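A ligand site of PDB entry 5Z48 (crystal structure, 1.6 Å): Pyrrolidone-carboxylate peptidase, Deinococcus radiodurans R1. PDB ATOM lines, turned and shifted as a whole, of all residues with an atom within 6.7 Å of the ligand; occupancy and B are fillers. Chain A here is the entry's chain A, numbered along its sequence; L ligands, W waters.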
ATOM      1  N   GLY A  10      16.824  20.237  14.154  1.00  0.00           N
ATOM      2  CA  GLY A  10      18.025  20.494  13.371  1.00  0.00           C
ATOM      3  C   GLY A  10      17.676  21.473  12.275  1.00  0.00           C
ATOM      4  O   GLY A  10      16.509  21.846  12.116  1.00  0.00           O
ATOM      5  N   PHE A  11      18.688  21.899  11.528  1.00  0.00           N
ATOM      6  CA  PHE A  11      18.517  22.888  10.460  1.00  0.00           C
ATOM      7  C   PHE A  11      18.847  22.283   9.106  1.00  0.00           C
ATOM      8  O   PHE A  11      19.685  21.368   9.002  1.00  0.00           O
ATOM      9  CB  PHE A  11      19.430  24.112  10.670  1.00  0.00           C
ATOM     10  CG  PHE A  11      18.864  25.148  11.565  1.00  0.00           C
ATOM     11  CD1 PHE A  11      17.871  26.021  11.094  1.00  0.00           C
ATOM     12  CD2 PHE A  11      19.324  25.278  12.873  1.00  0.00           C
ATOM     13  CE1 PHE A  11      17.364  26.976  11.916  1.00  0.00           C
ATOM     14  CE2 PHE A  11      18.842  26.254  13.734  1.00  0.00           C
ATOM     15  CZ  PHE A  11      17.846  27.126  13.229  1.00  0.00           C
ATOM     16  N   GLU A  12      18.207  22.826   8.041  1.00  0.00           N
ATOM     17  CA  GLU A  12      18.556  22.506   6.637  1.00  0.00           C
ATOM     18  C   GLU A  12      19.965  22.964   6.239  1.00  0.00           C
ATOM     19  O   GLU A  12      20.597  23.808   6.914  1.00  0.00           O
ATOM     20  CB  GLU A  12      17.534  23.136   5.692  1.00  0.00           C
ATOM     21  CG  GLU A  12      16.139  22.629   5.933  1.00  0.00           C
ATOM     22  CD  GLU A  12      15.060  23.296   5.072  1.00  0.00           C
ATOM     23  OE1 GLU A  12      15.323  24.221   4.253  1.00  0.00           O
ATOM     24  OE2 GLU A  12      13.892  22.876   5.256  1.00  0.00           O
ATOM     25  N   PHE A  14      22.728  25.215   4.341  1.00  0.00           N
ATOM     26  CA  PHE A  14      22.738  26.647   4.056  1.00  0.00           C
ATOM     27  C   PHE A  14      24.120  27.034   3.573  1.00  0.00           C
ATOM     28  O   PHE A  14      25.086  26.271   3.685  1.00  0.00           O
ATOM     29  CB  PHE A  14      22.350  27.445   5.305  1.00  0.00           C
ATOM     30  CG  PHE A  14      23.348  27.296   6.422  1.00  0.00           C
ATOM     31  CD1 PHE A  14      23.358  26.125   7.190  1.00  0.00           C
ATOM     32  CD2 PHE A  14      24.299  28.287   6.655  1.00  0.00           C
ATOM     33  CE1 PHE A  14      24.314  25.941   8.203  1.00  0.00           C
ATOM     34  CE2 PHE A  14      25.274  28.121   7.641  1.00  0.00           C
ATOM     35  CZ  PHE A  14      25.266  26.928   8.411  1.00  0.00           C
ATOM     36  N   ASN A  20      23.732  19.228   6.340  1.00  0.00           N
ATOM     37  CA  ASN A  20      23.747  19.813   7.666  1.00  0.00           C
ATOM     38  C   ASN A  20      23.728  18.667   8.673  1.00  0.00           C
ATOM     39  O   ASN A  20      22.730  17.922   8.745  1.00  0.00           O
ATOM     40  CB  ASN A  20      22.587  20.776   7.886  1.00  0.00           C
ATOM     41  CG  ASN A  20      22.771  21.623   9.117  1.00  0.00           C
ATOM     42  OD1 ASN A  20      23.201  21.112  10.146  1.00  0.00           O
ATOM     43  ND2 ASN A  20      22.463  22.903   9.030  1.00  0.00           N
ATOM     44  N   SER A  22      23.237  18.624  11.761  1.00  0.00           N
ATOM     45  CA  SER A  22      22.154  18.714  12.736  1.00  0.00           C
ATOM     46  C   SER A  22      20.862  18.135  12.172  1.00  0.00           C
ATOM     47  O   SER A  22      20.094  17.507  12.895  1.00  0.00           O
ATOM     48  CB  SER A  22      21.979  20.166  13.202  1.00  0.00           C
ATOM     49  OG  SER A  22      21.443  21.041  12.194  1.00  0.00           O
ATOM     50  N   PRO A  46      13.936  25.642   8.742  1.00  0.00           N
ATOM     51  CA  PRO A  46      14.621  26.321   7.638  1.00  0.00           C
ATOM     52  C   PRO A  46      15.613  27.338   8.190  1.00  0.00           C
ATOM     53  O   PRO A  46      15.449  27.846   9.287  1.00  0.00           O
ATOM     54  CB  PRO A  46      13.489  27.016   6.892  1.00  0.00           C
ATOM     55  CG  PRO A  46      12.468  27.315   7.982  1.00  0.00           C
ATOM     56  CD  PRO A  46      12.554  26.136   8.939  1.00  0.00           C
ATOM     57  N   VAL A  47      16.657  27.634   7.393  1.00  0.00           N
ATOM     58  CA  VAL A  47      17.644  28.638   7.806  1.00  0.00           C
ATOM     59  C   VAL A  47      17.190  30.013   7.359  1.00  0.00           C
ATOM     60  O   VAL A  47      17.743  30.628   6.430  1.00  0.00           O
ATOM     61  CB  VAL A  47      19.033  28.293   7.267  1.00  0.00           C
ATOM     62  CG1 VAL A  47      20.104  29.231   7.816  1.00  0.00           C
ATOM     63  CG2 VAL A  47      19.373  26.884   7.670  1.00  0.00           C
ATOM     64  N   THR A  71      19.415  22.075  17.749  1.00  0.00           N
ATOM     65  CA  THR A  71      20.783  21.792  17.282  1.00  0.00           C
ATOM     66  C   THR A  71      21.072  22.471  15.939  1.00  0.00           C
ATOM     67  O   THR A  71      20.167  22.807  15.169  1.00  0.00           O
ATOM     68  CB  THR A  71      21.077  20.265  17.173  1.00  0.00           C
ATOM     69  OG1 THR A  71      20.426  19.675  16.036  1.00  0.00           O
ATOM     70  CG2 THR A  71      20.657  19.530  18.475  1.00  0.00           C
ATOM     71  N   GLY A  72      22.367  22.641  15.626  1.00  0.00           N
ATOM     72  CA  GLY A  72      22.739  23.314  14.390  1.00  0.00           C
ATOM     73  C   GLY A  72      24.232  23.125  14.161  1.00  0.00           C
ATOM     74  O   GLY A  72      24.965  22.723  15.067  1.00  0.00           O
ATOM     75  N   LEU A  73      24.646  23.442  12.937  1.00  0.00           N
ATOM     76  CA  LEU A  73      26.034  23.334  12.482  1.00  0.00           C
ATOM     77  C   LEU A  73      26.825  24.563  12.914  1.00  0.00           C
ATOM     78  O   LEU A  73      26.382  25.692  12.718  1.00  0.00           O
ATOM     79  CB  LEU A  73      26.058  23.198  10.967  1.00  0.00           C
ATOM     80  CG  LEU A  73      27.424  23.308  10.248  1.00  0.00           C
ATOM     81  CD1 LEU A  73      28.385  22.185  10.681  1.00  0.00           C
ATOM     82  CD2 LEU A  73      27.216  23.298   8.732  1.00  0.00           C
ATOM     83  N   ALA A  74      28.023  24.332  13.462  1.00  0.00           N
ATOM     84  CA  ALA A  74      28.999  25.395  13.701  1.00  0.00           C
ATOM     85  C   ALA A  74      30.266  25.001  12.946  1.00  0.00           C
ATOM     86  O   ALA A  74      31.221  24.487  13.542  1.00  0.00           O
ATOM     87  CB  ALA A  74      29.277  25.609  15.201  1.00  0.00           C
ATOM     88  N   ALA A  75      30.272  25.245  11.631  1.00  0.00           N
ATOM     89  CA  ALA A  75      31.416  24.833  10.817  1.00  0.00           C
ATOM     90  C   ALA A  75      32.674  25.598  11.228  1.00  0.00           C
ATOM     91  O   ALA A  75      32.715  26.841  11.211  1.00  0.00           O
ATOM     92  CB  ALA A  75      31.115  25.032   9.321  1.00  0.00           C
ATOM     93  N   ALA A 141      26.512  32.014  20.586  1.00  0.00           N
ATOM     94  CA  ALA A 141      25.951  31.175  19.533  1.00  0.00           C
ATOM     95  C   ALA A 141      26.018  31.833  18.158  1.00  0.00           C
ATOM     96  O   ALA A 141      25.395  31.326  17.212  1.00  0.00           O
ATOM     97  CB  ALA A 141      24.495  30.827  19.868  1.00  0.00           C
ATOM     98  N   GLY A 142      26.767  32.955  18.044  1.00  0.00           N
ATOM     99  CA  GLY A 142      26.632  33.852  16.900  1.00  0.00           C
ATOM    100  C   GLY A 142      25.350  34.648  17.034  1.00  0.00           C
ATOM    101  O   GLY A 142      24.657  34.572  18.024  1.00  0.00           O
ATOM    102  N   LEU A 143      25.067  35.467  16.000  1.00  0.00           N
ATOM    103  CA  LEU A 143      23.813  36.234  15.941  1.00  0.00           C
ATOM    104  C   LEU A 143      23.045  35.913  14.645  1.00  0.00           C
ATOM    105  O   LEU A 143      22.266  36.716  14.152  1.00  0.00           O
ATOM    106  CB  LEU A 143      24.082  37.746  16.110  1.00  0.00           C
ATOM    107  CG  LEU A 143      24.716  38.177  17.444  1.00  0.00           C
ATOM    108  CD1 LEU A 143      24.927  39.675  17.431  1.00  0.00           C
ATOM    109  CD2 LEU A 143      23.836  37.767  18.634  1.00  0.00           C
ATOM    110  N   TYR A 144      23.222  34.688  14.145  1.00  0.00           N
ATOM    111  CA  TYR A 144      22.588  34.192  12.932  1.00  0.00           C
ATOM    112  C   TYR A 144      21.346  33.398  13.331  1.00  0.00           C
ATOM    113  O   TYR A 144      20.715  33.709  14.357  1.00  0.00           O
ATOM    114  CB  TYR A 144      23.637  33.393  12.111  1.00  0.00           C
ATOM    115  CG  TYR A 144      23.332  32.979  10.652  1.00  0.00           C
ATOM    116  CD1 TYR A 144      22.893  33.866   9.691  1.00  0.00           C
ATOM    117  CD2 TYR A 144      23.576  31.698  10.254  1.00  0.00           C
ATOM    118  CE1 TYR A 144      22.689  33.443   8.352  1.00  0.00           C
ATOM    119  CE2 TYR A 144      23.367  31.265   8.949  1.00  0.00           C
ATOM    120  CZ  TYR A 144      22.933  32.130   7.992  1.00  0.00           C
ATOM    121  OH  TYR A 144      22.750  31.715   6.701  1.00  0.00           O
ATOM    122  N   VAL A 145      20.950  32.394  12.555  1.00  0.00           N
ATOM    123  CA  VAL A 145      19.620  31.818  12.791  1.00  0.00           C
ATOM    124  C   VAL A 145      19.612  30.872  14.016  1.00  0.00           C
ATOM    125  O   VAL A 145      18.571  30.709  14.674  1.00  0.00           O
ATOM    126  CB  VAL A 145      19.097  31.119  11.504  1.00  0.00           C
ATOM    127  CG1 VAL A 145      17.590  30.697  11.650  1.00  0.00           C
ATOM    128  CG2 VAL A 145      19.220  32.012  10.265  1.00  0.00           C
ATOM    129  N   CYS A 146      20.715  30.169  14.305  1.00  0.00           N
ATOM    130  CA  CYS A 146      20.766  29.326  15.505  1.00  0.00           C
ATOM    131  C   CYS A 146      20.557  30.134  16.783  1.00  0.00           C
ATOM    132  O   CYS A 146      19.764  29.762  17.665  1.00  0.00           O
ATOM    133  CB  CYS A 146      22.096  28.571  15.564  1.00  0.00           C
ATOM    134  SG  CYS A 146      22.276  27.293  14.293  1.00  0.00           S
ATOM    135  N   ASN A 147      21.283  31.249  16.908  1.00  0.00           N
ATOM    136  CA  ASN A 147      21.025  32.114  18.053  1.00  0.00           C
ATOM    137  C   ASN A 147      19.590  32.591  18.076  1.00  0.00           C
ATOM    138  O   ASN A 147      18.967  32.651  19.147  1.00  0.00           O
ATOM    139  CB  ASN A 147      21.936  33.342  17.989  1.00  0.00           C
ATOM    140  CG  ASN A 147      21.665  34.348  19.108  1.00  0.00           C
ATOM    141  OD1 ASN A 147      22.110  34.128  20.252  1.00  0.00           O
ATOM    142  ND2 ASN A 147      20.927  35.413  18.801  1.00  0.00           N
ATOM    143  N   PHE A 148      19.052  32.971  16.906  1.00  0.00           N
ATOM    144  CA  PHE A 148      17.686  33.455  16.840  1.00  0.00           C
ATOM    145  C   PHE A 148      16.724  32.441  17.432  1.00  0.00           C
ATOM    146  O   PHE A 148      15.825  32.812  18.205  1.00  0.00           O
ATOM    147  CB  PHE A 148      17.295  33.794  15.391  1.00  0.00           C
ATOM    148  CG  PHE A 148      15.836  34.032  15.226  1.00  0.00           C
ATOM    149  CD1 PHE A 148      15.326  35.317  15.356  1.00  0.00           C
ATOM    150  CD2 PHE A 148      14.970  32.975  14.911  1.00  0.00           C
ATOM    151  CE1 PHE A 148      13.935  35.516  15.228  1.00  0.00           C
ATOM    152  CE2 PHE A 148      13.602  33.165  14.781  1.00  0.00           C
ATOM    153  CZ  PHE A 148      13.100  34.455  14.931  1.00  0.00           C
ATOM    154  N   PHE A 169      20.641  25.030  23.323  1.00  0.00           N
ATOM    155  CA  PHE A 169      21.186  24.845  21.983  1.00  0.00           C
ATOM    156  C   PHE A 169      22.473  24.047  22.007  1.00  0.00           C
ATOM    157  O   PHE A 169      23.345  24.259  22.856  1.00  0.00           O
ATOM    158  CB  PHE A 169      21.450  26.222  21.259  1.00  0.00           C
ATOM    159  CG  PHE A 169      21.434  26.083  19.752  1.00  0.00           C
ATOM    160  CD1 PHE A 169      22.575  25.634  19.067  1.00  0.00           C
ATOM    161  CD2 PHE A 169      20.262  26.309  19.040  1.00  0.00           C
ATOM    162  CE1 PHE A 169      22.504  25.401  17.700  1.00  0.00           C
ATOM    163  CE2 PHE A 169      20.190  26.105  17.681  1.00  0.00           C
ATOM    164  CZ  PHE A 169      21.310  25.620  17.009  1.00  0.00           C
ATOM    165  N   HIS A 171      25.483  23.125  19.341  1.00  0.00           N
ATOM    166  CA  HIS A 171      26.149  23.303  18.059  1.00  0.00           C
ATOM    167  C   HIS A 171      27.075  22.121  17.807  1.00  0.00           C
ATOM    168  O   HIS A 171      27.805  21.692  18.696  1.00  0.00           O
ATOM    169  CB  HIS A 171      26.980  24.592  18.062  1.00  0.00           C
ATOM    170  CG  HIS A 171      26.327  25.771  17.399  1.00  0.00           C
ATOM    171  ND1 HIS A 171      26.187  26.992  18.027  1.00  0.00           N
ATOM    172  CD2 HIS A 171      25.802  25.933  16.154  1.00  0.00           C
ATOM    173  CE1 HIS A 171      25.624  27.856  17.202  1.00  0.00           C
ATOM    174  NE2 HIS A 171      25.399  27.247  16.043  1.00  0.00           N
HETATM  175  N1  LIG L   1      24.097  26.831  11.673  1.00  0.00           N
HETATM  176  C1  LIG L   1      23.823  28.265  11.449  1.00  0.00           C
HETATM  177  C2  LIG L   1      22.401  28.379  10.879  1.00  0.00           C
HETATM  178  C3  LIG L   1      21.886  26.957  10.615  1.00  0.00           C
HETATM  179  C4  LIG L   1      22.992  26.090  11.193  1.00  0.00           C
HETATM  180  O1  LIG L   1      22.896  24.832  11.256  1.00  0.00           O
HETATM  181  C5  LIG L   1      24.066  29.066  12.742  1.00  0.00           C
HETATM  182  O2  LIG L   1      23.439  30.098  13.013  1.00  0.00           O
HETATM  183  O3  LIG L   1      24.889  28.663  13.626  1.00  0.00           O
HETATM  184  O   HOH W   1      27.585  28.720  12.244  1.00  0.00           O
HETATM  185  O   HOH W   2      23.631  31.919  15.181  1.00  0.00           O
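The side-chain amide nitrogen (ND2) of Asn 20 sits at hydrogen-bond distance from the backbone carbonyl oxygen (O) of Glu 12 (3.0 Å).
N of Phe 11 is in hydrogen-bond range of OG of Ser 22 (3.0 Å).
ND2 of Asn 20 sits close to O of Phe 11 (3.2 Å).
A ring nitrogen (NE2) of His 171 sits at hydrogen-bond distance from the side-chain sulfur (SG) of Cys 146 (3.6 Å).
The side-chain amide oxygen of Asn 20 is in hydrogen-bond range of the side-chain hydroxyl of Ser 22 (2.7 Å).
The backbone NH (N) of Leu 73 sits at hydrogen-bond distance from an oxygen (O1) of the ligand, at 2.8 Å.
The backbone carbonyl oxygen of Leu 73 is in hydrogen-bond range of a nitrogen (N1) of the ligand.
The backbone NH (N) of Cys 146 lies within hydrogen-bond range of an oxygen (O2) of the ligand, 3.0 Å away.
O2 of the ligand lies within hydrogen-bond range of N of Val 145, at 3.4 Å.
O3 of the ligand lies close to SG of Cys 146 (3.0 Å).
The side-chain amide nitrogen (ND2) of Asn 20 lies within hydrogen-bond range of an oxygen (O1) of the ligand, 3.0 Å away.
An oxygen (O3) of the ligand sits at hydrogen-bond distance from a ring nitrogen (NE2) of His 171 (2.8 Å).
Water W2 lies within hydrogen-bond range of the backbone carbonyl oxygen of Ala 141 (2.8 Å), an oxygen (O2) of the ligand (2.8 Å), the backbone NH of Tyr 144 (3.0 Å) and the backbone NH of Asn 147 (3.0 Å).
Water W1 lies within hydrogen-bond range of O3 of the ligand (3.0 Å) and O of Leu 73 (3.3 Å).
Phe 11 touches the ligand.
Phe 14 touches the ligand.
Val 47 touches the ligand.
CA of Gly 72 touches O1 of the ligand, at 3.5 Å.
CD2 of Tyr 144 touches O2 of the ligand (3.2 Å).
Hydrophobic or aromatic side chains that line the ligand: Phe 11, Phe 14, Val 47, Leu 73, Tyr 144 and His 171.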
